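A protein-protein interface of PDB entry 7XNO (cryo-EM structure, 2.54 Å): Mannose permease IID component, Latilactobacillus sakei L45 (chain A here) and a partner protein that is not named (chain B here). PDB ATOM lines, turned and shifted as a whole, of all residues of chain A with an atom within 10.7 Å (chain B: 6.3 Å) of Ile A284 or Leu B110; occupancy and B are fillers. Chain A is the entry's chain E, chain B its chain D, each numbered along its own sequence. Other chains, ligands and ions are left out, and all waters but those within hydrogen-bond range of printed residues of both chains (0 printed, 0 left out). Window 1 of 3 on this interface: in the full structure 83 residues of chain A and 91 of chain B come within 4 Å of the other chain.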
ATOM      1  N   TRP A  26       5.577  -2.284   2.330  1.00  0.00           N
ATOM      2  CA  TRP A  26       6.329  -1.600   3.378  1.00  0.00           C
ATOM      3  C   TRP A  26       7.777  -1.355   2.934  1.00  0.00           C
ATOM      4  O   TRP A  26       8.717  -1.979   3.419  1.00  0.00           O
ATOM      5  CB  TRP A  26       6.328  -2.372   4.700  1.00  0.00           C
ATOM      6  CG  TRP A  26       6.732  -1.481   5.848  1.00  0.00           C
ATOM      7  CD1 TRP A  26       5.943  -0.543   6.442  1.00  0.00           C
ATOM      8  CD2 TRP A  26       8.039  -1.317   6.422  1.00  0.00           C
ATOM      9  NE1 TRP A  26       6.641   0.125   7.412  1.00  0.00           N
ATOM     10  CE2 TRP A  26       7.934  -0.322   7.412  1.00  0.00           C
ATOM     11  CE3 TRP A  26       9.272  -1.939   6.226  1.00  0.00           C
ATOM     12  CZ2 TRP A  26       9.013   0.066   8.197  1.00  0.00           C
ATOM     13  CZ3 TRP A  26      10.342  -1.548   7.005  1.00  0.00           C
ATOM     14  CH2 TRP A  26      10.205  -0.561   7.979  1.00  0.00           C
ATOM     15  N   TYR A  28      11.121   1.243   2.470  1.00  0.00           N
ATOM     16  CA  TYR A  28      11.812   2.032   3.481  1.00  0.00           C
ATOM     17  C   TYR A  28      11.644   3.536   3.307  1.00  0.00           C
ATOM     18  O   TYR A  28      11.928   4.284   4.249  1.00  0.00           O
ATOM     19  CB  TYR A  28      13.305   1.685   3.494  1.00  0.00           C
ATOM     20  CG  TYR A  28      13.658   0.605   4.491  1.00  0.00           C
ATOM     21  CD1 TYR A  28      13.433   0.788   5.848  1.00  0.00           C
ATOM     22  CD2 TYR A  28      14.209  -0.598   4.076  1.00  0.00           C
ATOM     23  CE1 TYR A  28      13.748  -0.195   6.763  1.00  0.00           C
ATOM     24  CE2 TYR A  28      14.529  -1.588   4.986  1.00  0.00           C
ATOM     25  CZ  TYR A  28      14.296  -1.381   6.327  1.00  0.00           C
ATOM     26  OH  TYR A  28      14.611  -2.361   7.239  1.00  0.00           O
ATOM     27  N   CYS A 273      27.059   1.809  22.774  1.00  0.00           N
ATOM     28  CA  CYS A 273      26.100   1.539  21.707  1.00  0.00           C
ATOM     29  C   CYS A 273      25.454   2.826  21.207  1.00  0.00           C
ATOM     30  O   CYS A 273      25.228   2.984  20.003  1.00  0.00           O
ATOM     31  CB  CYS A 273      25.035   0.557  22.195  1.00  0.00           C
ATOM     32  SG  CYS A 273      25.600  -1.153  22.323  1.00  0.00           S
ATOM     33  N   LEU A 276      28.014   4.475  18.993  1.00  0.00           N
ATOM     34  CA  LEU A 276      28.118   3.770  17.720  1.00  0.00           C
ATOM     35  C   LEU A 276      26.928   4.073  16.819  1.00  0.00           C
ATOM     36  O   LEU A 276      27.094   4.265  15.609  1.00  0.00           O
ATOM     37  CB  LEU A 276      28.235   2.266  17.960  1.00  0.00           C
ATOM     38  CG  LEU A 276      29.565   1.753  18.510  1.00  0.00           C
ATOM     39  CD1 LEU A 276      29.483   0.263  18.789  1.00  0.00           C
ATOM     40  CD2 LEU A 276      30.696   2.061  17.545  1.00  0.00           C
ATOM     41  N   LEU A 277      25.720   4.110  17.386  1.00  0.00           N
ATOM     42  CA  LEU A 277      24.540   4.448  16.599  1.00  0.00           C
ATOM     43  C   LEU A 277      24.625   5.870  16.065  1.00  0.00           C
ATOM     44  O   LEU A 277      24.221   6.141  14.928  1.00  0.00           O
ATOM     45  CB  LEU A 277      23.275   4.267  17.437  1.00  0.00           C
ATOM     46  CG  LEU A 277      22.835   2.833  17.731  1.00  0.00           C
ATOM     47  CD1 LEU A 277      21.742   2.823  18.784  1.00  0.00           C
ATOM     48  CD2 LEU A 277      22.365   2.143  16.462  1.00  0.00           C
ATOM     49  N   LYS A 280      26.483   6.418  12.668  1.00  0.00           N
ATOM     50  CA  LYS A 280      25.907   5.818  11.462  1.00  0.00           C
ATOM     51  C   LYS A 280      26.294   4.349  11.303  1.00  0.00           C
ATOM     52  O   LYS A 280      26.395   3.843  10.184  1.00  0.00           O
ATOM     53  CB  LYS A 280      26.292   6.608  10.208  1.00  0.00           C
ATOM     54  CG  LYS A 280      25.948   8.086  10.281  1.00  0.00           C
ATOM     55  CD  LYS A 280      26.308   8.803   8.993  1.00  0.00           C
ATOM     56  CE  LYS A 280      26.057  10.296   9.109  1.00  0.00           C
ATOM     57  NZ  LYS A 280      26.763  10.883  10.281  1.00  0.00           N
ATOM     58  N   VAL A 281      26.512   3.654  12.414  1.00  0.00           N
ATOM     59  CA  VAL A 281      26.718   2.210  12.381  1.00  0.00           C
ATOM     60  C   VAL A 281      25.363   1.525  12.498  1.00  0.00           C
ATOM     61  O   VAL A 281      24.573   1.837  13.397  1.00  0.00           O
ATOM     62  CB  VAL A 281      27.668   1.766  13.504  1.00  0.00           C
ATOM     63  CG1 VAL A 281      27.944   0.276  13.408  1.00  0.00           C
ATOM     64  CG2 VAL A 281      28.967   2.554  13.442  1.00  0.00           C
ATOM     65  N   SER A 282      25.087   0.600  11.583  1.00  0.00           N
ATOM     66  CA  SER A 282      23.779  -0.038  11.548  1.00  0.00           C
ATOM     67  C   SER A 282      23.574  -0.903  12.790  1.00  0.00           C
ATOM     68  O   SER A 282      24.517  -1.541  13.267  1.00  0.00           O
ATOM     69  CB  SER A 282      23.628  -0.887  10.288  1.00  0.00           C
ATOM     70  OG  SER A 282      24.550  -1.959  10.284  1.00  0.00           O
ATOM     71  N   PRO A 283      22.359  -0.934  13.343  1.00  0.00           N
ATOM     72  CA  PRO A 283      22.126  -1.723  14.564  1.00  0.00           C
ATOM     73  C   PRO A 283      22.345  -3.215  14.387  1.00  0.00           C
ATOM     74  O   PRO A 283      22.687  -3.897  15.360  1.00  0.00           O
ATOM     75  CB  PRO A 283      20.664  -1.406  14.912  1.00  0.00           C
ATOM     76  CG  PRO A 283      20.349  -0.145  14.174  1.00  0.00           C
ATOM     77  CD  PRO A 283      21.160  -0.190  12.925  1.00  0.00           C
ATOM     78  N   ILE A 284      22.149  -3.751  13.180  1.00  0.00           N
ATOM     79  CA  ILE A 284      22.330  -5.184  12.970  1.00  0.00           C
ATOM     80  C   ILE A 284      23.800  -5.564  13.115  1.00  0.00           C
ATOM     81  O   ILE A 284      24.133  -6.626  13.660  1.00  0.00           O
ATOM     82  CB  ILE A 284      21.748  -5.601  11.605  1.00  0.00           C
ATOM     83  CG1 ILE A 284      21.787  -7.122  11.442  1.00  0.00           C
ATOM     84  CG2 ILE A 284      22.460  -4.896  10.456  1.00  0.00           C
ATOM     85  CD1 ILE A 284      20.704  -7.840  12.210  1.00  0.00           C
ATOM     86  N   VAL A 285      24.701  -4.697  12.646  1.00  0.00           N
ATOM     87  CA  VAL A 285      26.128  -4.916  12.855  1.00  0.00           C
ATOM     88  C   VAL A 285      26.446  -4.927  14.342  1.00  0.00           C
ATOM     89  O   VAL A 285      27.241  -5.745  14.814  1.00  0.00           O
ATOM     90  CB  VAL A 285      26.949  -3.852  12.101  1.00  0.00           C
ATOM     91  CG1 VAL A 285      28.385  -3.836  12.591  1.00  0.00           C
ATOM     92  CG2 VAL A 285      26.907  -4.116  10.608  1.00  0.00           C
ATOM     93  N   ILE A 286      25.818  -4.032  15.106  1.00  0.00           N
ATOM     94  CA  ILE A 286      26.062  -3.980  16.544  1.00  0.00           C
ATOM     95  C   ILE A 286      25.548  -5.244  17.226  1.00  0.00           C
ATOM     96  O   ILE A 286      26.181  -5.765  18.147  1.00  0.00           O
ATOM     97  CB  ILE A 286      25.431  -2.713  17.148  1.00  0.00           C
ATOM     98  CG1 ILE A 286      25.860  -1.477  16.358  1.00  0.00           C
ATOM     99  CG2 ILE A 286      25.832  -2.563  18.604  1.00  0.00           C
ATOM    100  CD1 ILE A 286      25.334  -0.178  16.924  1.00  0.00           C
ATOM    101  N   ILE A 287      24.396  -5.756  16.789  1.00  0.00           N
ATOM    102  CA  ILE A 287      23.847  -6.974  17.384  1.00  0.00           C
ATOM    103  C   ILE A 287      24.759  -8.166  17.104  1.00  0.00           C
ATOM    104  O   ILE A 287      25.076  -8.961  18.002  1.00  0.00           O
ATOM    105  CB  ILE A 287      22.418  -7.218  16.870  1.00  0.00           C
ATOM    106  CG1 ILE A 287      21.465  -6.155  17.420  1.00  0.00           C
ATOM    107  CG2 ILE A 287      21.938  -8.608  17.251  1.00  0.00           C
ATOM    108  CD1 ILE A 287      20.241  -5.926  16.563  1.00  0.00           C
ATOM    109  N   LEU A 288      25.199  -8.305  15.849  1.00  0.00           N
ATOM    110  CA  LEU A 288      26.116  -9.389  15.510  1.00  0.00           C
ATOM    111  C   LEU A 288      27.431  -9.253  16.268  1.00  0.00           C
ATOM    112  O   LEU A 288      27.996 -10.249  16.738  1.00  0.00           O
ATOM    113  CB  LEU A 288      26.361  -9.412  14.002  1.00  0.00           C
ATOM    114  CG  LEU A 288      25.149  -9.760  13.137  1.00  0.00           C
ATOM    115  CD1 LEU A 288      25.426  -9.458  11.674  1.00  0.00           C
ATOM    116  CD2 LEU A 288      24.766 -11.217  13.322  1.00  0.00           C
ATOM    117  N   GLY A 289      27.928  -8.023  16.405  1.00  0.00           N
ATOM    118  CA  GLY A 289      29.144  -7.808  17.165  1.00  0.00           C
ATOM    119  C   GLY A 289      28.983  -8.149  18.630  1.00  0.00           C
ATOM    120  O   GLY A 289      29.908  -8.655  19.259  1.00  0.00           O
ATOM    121  N   LEU A 290      27.807  -7.873  19.198  1.00  0.00           N
ATOM    122  CA  LEU A 290      27.558  -8.246  20.587  1.00  0.00           C
ATOM    123  C   LEU A 290      27.543  -9.758  20.754  1.00  0.00           C
ATOM    124  O   LEU A 290      28.077 -10.285  21.738  1.00  0.00           O
ATOM    125  CB  LEU A 290      26.244  -7.635  21.073  1.00  0.00           C
ATOM    126  CG  LEU A 290      26.307  -6.157  21.462  1.00  0.00           C
ATOM    127  CD1 LEU A 290      24.944  -5.663  21.908  1.00  0.00           C
ATOM    128  CD2 LEU A 290      27.346  -5.932  22.548  1.00  0.00           C
ATOM    129  N   PHE A 291      26.946 -10.474  19.799  1.00  0.00           N
ATOM    130  CA  PHE A 291      26.998 -11.935  19.840  1.00  0.00           C
ATOM    131  C   PHE A 291      28.441 -12.431  19.776  1.00  0.00           C
ATOM    132  O   PHE A 291      28.845 -13.327  20.533  1.00  0.00           O
ATOM    133  CB  PHE A 291      26.177 -12.524  18.692  1.00  0.00           C
ATOM    134  CG  PHE A 291      24.718 -12.682  19.008  1.00  0.00           C
ATOM    135  CD1 PHE A 291      24.292 -13.637  19.914  1.00  0.00           C
ATOM    136  CD2 PHE A 291      23.773 -11.879  18.394  1.00  0.00           C
ATOM    137  CE1 PHE A 291      22.950 -13.786  20.205  1.00  0.00           C
ATOM    138  CE2 PHE A 291      22.431 -12.023  18.681  1.00  0.00           C
ATOM    139  CZ  PHE A 291      22.018 -12.978  19.587  1.00  0.00           C
ATOM    140  N   VAL A 292      29.237 -11.843  18.879  1.00  0.00           N
ATOM    141  CA  VAL A 292      30.630 -12.258  18.724  1.00  0.00           C
ATOM    142  C   VAL A 292      31.427 -11.956  19.989  1.00  0.00           C
ATOM    143  O   VAL A 292      32.263 -12.760  20.419  1.00  0.00           O
ATOM    144  CB  VAL A 292      31.248 -11.586  17.485  1.00  0.00           C
ATOM    145  CG1 VAL A 292      32.760 -11.748  17.478  1.00  0.00           C
ATOM    146  CG2 VAL A 292      30.642 -12.162  16.217  1.00  0.00           C
ATOM    147  N   VAL B  70      13.117  -2.707  12.755  1.00  0.00           N
ATOM    148  CA  VAL B  70      12.491  -4.021  12.644  1.00  0.00           C
ATOM    149  C   VAL B  70      12.983  -4.923  13.767  1.00  0.00           C
ATOM    150  O   VAL B  70      14.179  -4.957  14.079  1.00  0.00           O
ATOM    151  CB  VAL B  70      12.776  -4.649  11.267  1.00  0.00           C
ATOM    152  CG1 VAL B  70      11.934  -5.897  11.066  1.00  0.00           C
ATOM    153  CG2 VAL B  70      12.514  -3.639  10.162  1.00  0.00           C
ATOM    154  N   ALA B  71      12.052  -5.653  14.379  1.00  0.00           N
ATOM    155  CA  ALA B  71      12.373  -6.596  15.436  1.00  0.00           C
ATOM    156  C   ALA B  71      13.005  -7.861  14.854  1.00  0.00           C
ATOM    157  O   ALA B  71      12.919  -8.112  13.650  1.00  0.00           O
ATOM    158  CB  ALA B  71      11.110  -6.944  16.220  1.00  0.00           C
ATOM    159  N   PRO B  72      13.661  -8.681  15.697  1.00  0.00           N
ATOM    160  CA  PRO B  72      14.375  -9.854  15.167  1.00  0.00           C
ATOM    161  C   PRO B  72      13.501 -11.004  14.680  1.00  0.00           C
ATOM    162  O   PRO B  72      13.668 -12.129  15.154  1.00  0.00           O
ATOM    163  CB  PRO B  72      15.232 -10.305  16.359  1.00  0.00           C
ATOM    164  CG  PRO B  72      15.325  -9.121  17.247  1.00  0.00           C
ATOM    165  CD  PRO B  72      14.024  -8.415  17.100  1.00  0.00           C
ATOM    166  N   ASP B  73      12.569 -10.739  13.761  1.00  0.00           N
ATOM    167  CA  ASP B  73      12.004 -11.753  12.869  1.00  0.00           C
ATOM    168  C   ASP B  73      11.625 -13.078  13.525  1.00  0.00           C
ATOM    169  O   ASP B  73      12.273 -14.097  13.270  1.00  0.00           O
ATOM    170  CB  ASP B  73      12.966 -12.043  11.720  1.00  0.00           C
ATOM    171  CG  ASP B  73      12.252 -12.573  10.494  1.00  0.00           C
ATOM    172  OD1 ASP B  73      11.291 -11.922  10.037  1.00  0.00           O
ATOM    173  OD2 ASP B  73      12.633 -13.650   9.997  1.00  0.00           O
ATOM    174  N   LEU B  76      11.120 -16.540  11.002  1.00  0.00           N
ATOM    175  CA  LEU B  76      12.161 -17.473  10.579  1.00  0.00           C
ATOM    176  C   LEU B  76      12.672 -18.295  11.749  1.00  0.00           C
ATOM    177  O   LEU B  76      12.897 -19.501  11.611  1.00  0.00           O
ATOM    178  CB  LEU B  76      13.322 -16.735   9.914  1.00  0.00           C
ATOM    179  CG  LEU B  76      14.349 -17.686   9.289  1.00  0.00           C
ATOM    180  CD1 LEU B  76      13.707 -18.529   8.199  1.00  0.00           C
ATOM    181  CD2 LEU B  76      15.556 -16.942   8.748  1.00  0.00           C
ATOM    182  N   LEU B 105      19.021 -17.590  14.324  1.00  0.00           N
ATOM    183  CA  LEU B 105      18.104 -17.659  13.193  1.00  0.00           C
ATOM    184  C   LEU B 105      17.204 -16.432  13.152  1.00  0.00           C
ATOM    185  O   LEU B 105      16.863 -15.937  12.073  1.00  0.00           O
ATOM    186  CB  LEU B 105      17.273 -18.938  13.272  1.00  0.00           C
ATOM    187  CG  LEU B 105      17.983 -20.220  12.835  1.00  0.00           C
ATOM    188  CD1 LEU B 105      17.223 -21.437  13.329  1.00  0.00           C
ATOM    189  CD2 LEU B 105      18.140 -20.259  11.326  1.00  0.00           C
ATOM    190  N   ALA B 106      16.818 -15.923  14.324  1.00  0.00           N
ATOM    191  CA  ALA B 106      16.032 -14.696  14.380  1.00  0.00           C
ATOM    192  C   ALA B 106      16.809 -13.514  13.814  1.00  0.00           C
ATOM    193  O   ALA B 106      16.256 -12.693  13.072  1.00  0.00           O
ATOM    194  CB  ALA B 106      15.604 -14.422  15.819  1.00  0.00           C
ATOM    195  N   VAL B 107      18.098 -13.413  14.144  1.00  0.00           N
ATOM    196  CA  VAL B 107      18.911 -12.317  13.618  1.00  0.00           C
ATOM    197  C   VAL B 107      19.106 -12.462  12.109  1.00  0.00           C
ATOM    198  O   VAL B 107      19.068 -11.473  11.362  1.00  0.00           O
ATOM    199  CB  VAL B 107      20.254 -12.247  14.365  1.00  0.00           C
ATOM    200  CG1 VAL B 107      21.097 -11.103  13.836  1.00  0.00           C
ATOM    201  CG2 VAL B 107      20.017 -12.086  15.856  1.00  0.00           C
ATOM    202  N   ALA B 108      19.316 -13.693  11.636  1.00  0.00           N
ATOM    203  CA  ALA B 108      19.438 -13.920  10.199  1.00  0.00           C
ATOM    204  C   ALA B 108      18.153 -13.547   9.470  1.00  0.00           C
ATOM    205  O   ALA B 108      18.190 -12.956   8.384  1.00  0.00           O
ATOM    206  CB  ALA B 108      19.809 -15.377   9.927  1.00  0.00           C
ATOM    207  N   GLY B 109      17.002 -13.885  10.054  1.00  0.00           N
ATOM    208  CA  GLY B 109      15.738 -13.482   9.470  1.00  0.00           C
ATOM    209  C   GLY B 109      15.528 -11.984   9.485  1.00  0.00           C
ATOM    210  O   GLY B 109      14.919 -11.433   8.566  1.00  0.00           O
ATOM    211  N   LEU B 110      16.010 -11.308  10.531  1.00  0.00           N
ATOM    212  CA  LEU B 110      15.971  -9.850  10.547  1.00  0.00           C
ATOM    213  C   LEU B 110      16.784  -9.273   9.395  1.00  0.00           C
ATOM    214  O   LEU B 110      16.343  -8.335   8.719  1.00  0.00           O
ATOM    215  CB  LEU B 110      16.485  -9.335  11.892  1.00  0.00           C
ATOM    216  CG  LEU B 110      16.801  -7.846  12.052  1.00  0.00           C
ATOM    217  CD1 LEU B 110      15.618  -6.982  11.649  1.00  0.00           C
ATOM    218  CD2 LEU B 110      17.221  -7.550  13.481  1.00  0.00           C
ATOM    219  N   LEU B 111      17.969  -9.831   9.148  1.00  0.00           N
ATOM    220  CA  LEU B 111      18.769  -9.390   8.007  1.00  0.00           C
ATOM    221  C   LEU B 111      18.032  -9.625   6.690  1.00  0.00           C
ATOM    222  O   LEU B 111      17.998  -8.747   5.813  1.00  0.00           O
ATOM    223  CB  LEU B 111      20.118 -10.111   8.017  1.00  0.00           C
ATOM    224  CG  LEU B 111      21.236  -9.646   7.083  1.00  0.00           C
ATOM    225  CD1 LEU B 111      22.581  -9.834   7.757  1.00  0.00           C
ATOM    226  CD2 LEU B 111      21.200 -10.408   5.769  1.00  0.00           C
ATOM    227  N   LEU B 112      17.422 -10.804   6.542  1.00  0.00           N
ATOM    228  CA  LEU B 112      16.702 -11.122   5.312  1.00  0.00           C
ATOM    229  C   LEU B 112      15.521 -10.183   5.095  1.00  0.00           C
ATOM    230  O   LEU B 112      15.272  -9.731   3.969  1.00  0.00           O
ATOM    231  CB  LEU B 112      16.226 -12.574   5.344  1.00  0.00           C
ATOM    232  CG  LEU B 112      17.246 -13.650   4.972  1.00  0.00           C
ATOM    233  CD1 LEU B 112      16.596 -15.022   4.991  1.00  0.00           C
ATOM    234  CD2 LEU B 112      17.854 -13.360   3.612  1.00  0.00           C
ATOM    235  N   THR B 113      14.776  -9.879   6.160  1.00  0.00           N
ATOM    236  CA  THR B 113      13.627  -8.997   6.006  1.00  0.00           C
ATOM    237  C   THR B 113      14.065  -7.562   5.757  1.00  0.00           C
ATOM    238  O   THR B 113      13.369  -6.829   5.052  1.00  0.00           O
ATOM    239  CB  THR B 113      12.696  -9.091   7.221  1.00  0.00           C
ATOM    240  OG1 THR B 113      11.433  -8.496   6.901  1.00  0.00           O
ATOM    241  CG2 THR B 113      13.273  -8.382   8.428  1.00  0.00           C
ATOM    242  N   ILE B 114      15.223  -7.152   6.282  1.00  0.00           N
ATOM    243  CA  ILE B 114      15.769  -5.850   5.911  1.00  0.00           C
ATOM    244  C   ILE B 114      16.058  -5.808   4.416  1.00  0.00           C
ATOM    245  O   ILE B 114      15.732  -4.830   3.729  1.00  0.00           O
ATOM    246  CB  ILE B 114      17.029  -5.537   6.740  1.00  0.00           C
ATOM    247  CG1 ILE B 114      16.651  -5.200   8.183  1.00  0.00           C
ATOM    248  CG2 ILE B 114      17.814  -4.395   6.117  1.00  0.00           C
ATOM    249  CD1 ILE B 114      17.838  -5.067   9.105  1.00  0.00           C
ATOM    250  N   ILE B 115      16.652  -6.879   3.885  1.00  0.00           N
ATOM    251  CA  ILE B 115      16.955  -6.926   2.455  1.00  0.00           C
ATOM    252  C   ILE B 115      15.672  -6.847   1.630  1.00  0.00           C
ATOM    253  O   ILE B 115      15.589  -6.103   0.643  1.00  0.00           O
ATOM    254  CB  ILE B 115      17.765  -8.189   2.118  1.00  0.00           C
ATOM    255  CG1 ILE B 115      19.179  -8.085   2.692  1.00  0.00           C
ATOM    256  CG2 ILE B 115      17.812  -8.412   0.615  1.00  0.00           C
ATOM    257  CD1 ILE B 115      20.020  -9.315   2.454  1.00  0.00           C
ATOM    258  N   ARG B 153      10.358 -15.223   1.072  1.00  0.00           N
ATOM    259  CA  ARG B 153      11.565 -14.982   1.860  1.00  0.00           C
ATOM    260  C   ARG B 153      11.738 -16.022   2.962  1.00  0.00           C
ATOM    261  O   ARG B 153      12.864 -16.417   3.281  1.00  0.00           O
ATOM    262  CB  ARG B 153      11.533 -13.582   2.477  1.00  0.00           C
ATOM    263  CG  ARG B 153      12.607 -13.369   3.540  1.00  0.00           C
ATOM    264  CD  ARG B 153      12.423 -12.080   4.306  1.00  0.00           C
ATOM    265  NE  ARG B 153      11.293 -12.149   5.225  1.00  0.00           N
ATOM    266  CZ  ARG B 153      11.398 -12.358   6.530  1.00  0.00           C
ATOM    267  NH1 ARG B 153      12.575 -12.521   7.112  1.00  0.00           N
ATOM    268  NH2 ARG B 153      10.295 -12.406   7.270  1.00  0.00           N
ATOM    269  N   VAL B 194      21.269  -2.519  22.503  1.00  0.00           N
ATOM    270  CA  VAL B 194      21.095  -1.799  21.244  1.00  0.00           C
ATOM    271  C   VAL B 194      19.737  -1.107  21.203  1.00  0.00           C
ATOM    272  O   VAL B 194      19.629   0.068  20.829  1.00  0.00           O
ATOM    273  CB  VAL B 194      21.275  -2.755  20.051  1.00  0.00           C
ATOM    274  CG1 VAL B 194      21.111  -2.006  18.739  1.00  0.00           C
ATOM    275  CG2 VAL B 194      22.628  -3.435  20.119  1.00  0.00           C
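CG2 of Val B70 touches OH of Tyr A28, 3.8 Å away. Ile B114 touches Tyr A28 (CG1 to OH, 3.6 Å). CB of Pro A283 touches CG1 of Val B194, at 3.9 Å. Val B107 touches Ile A284. CD2 of Leu B110 touches CD1 of Ile A284 (3.7 Å). Ile A286 touches Val B194 (CG2 to CG2, 3.6 Å). Val B107 touches Leu A288. Leu A290 touches Val B194 (CD1 to CG2, 3.7 Å). CG2 of Val B107 touches CE2 of Phe A291 (3.7 Å).
Of the printed residues of chain B, Tyr A28 touches Val B70 and Ile B114. Of the printed residues of chain B, Pro A283 touches Val B194 (3.9 Å). Ile A284 touches just these residues of chain B: Val B107 (3.7 Å) and Leu B110 (3.7 Å). Of the printed residues of chain B, Phe A291 touches Val B107. Val A292 touches none of the printed residues of chain B. No residue of chain A comes within 4 Å of Pro B72. Of chain A, only Ile A284, Leu A288 and Phe A291 come within 4 Å of Val B107. No residue of chain A comes within 4 Å of Ala B108. Leu B110 touches just one residue of chain A: Ile A284 (3.7 Å). Of the printed residues of chain A, Ile B114 touches Tyr A28 (3.6 Å). Of the printed residues of chain A, Val B194 touches Pro A283 (3.9 Å), Ile A286 (3.6 Å) and Leu A290 (3.7 Å). The nearest residue of chain B that does not touch Ile A284 is Leu B111 (4.6 Å). The nearest printed residue of chain B that does not touch Ile A286 is Val B107 (8.1 Å).
Hydrophobic or aromatic side chains of chain B that line the printed part of chain A: Val B70, Val B107, Leu B110, Ile B114 and Val B194. Of the 18 printed residues of chain A, 7 touch a printed residue of chain B. Hydrophobic or aromatic side chains of chain A that line the printed part of chain B: Tyr A28, Pro A283, Ile A284, Ile A286, Leu A288, Leu A290 and Phe A291. Among the printed residues, 9 pairs touch across the chains. Among the printed residues, no Asp or Glu carboxylate lies within 4 Å of a Lys or Arg side-chain nitrogen of the other chain.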
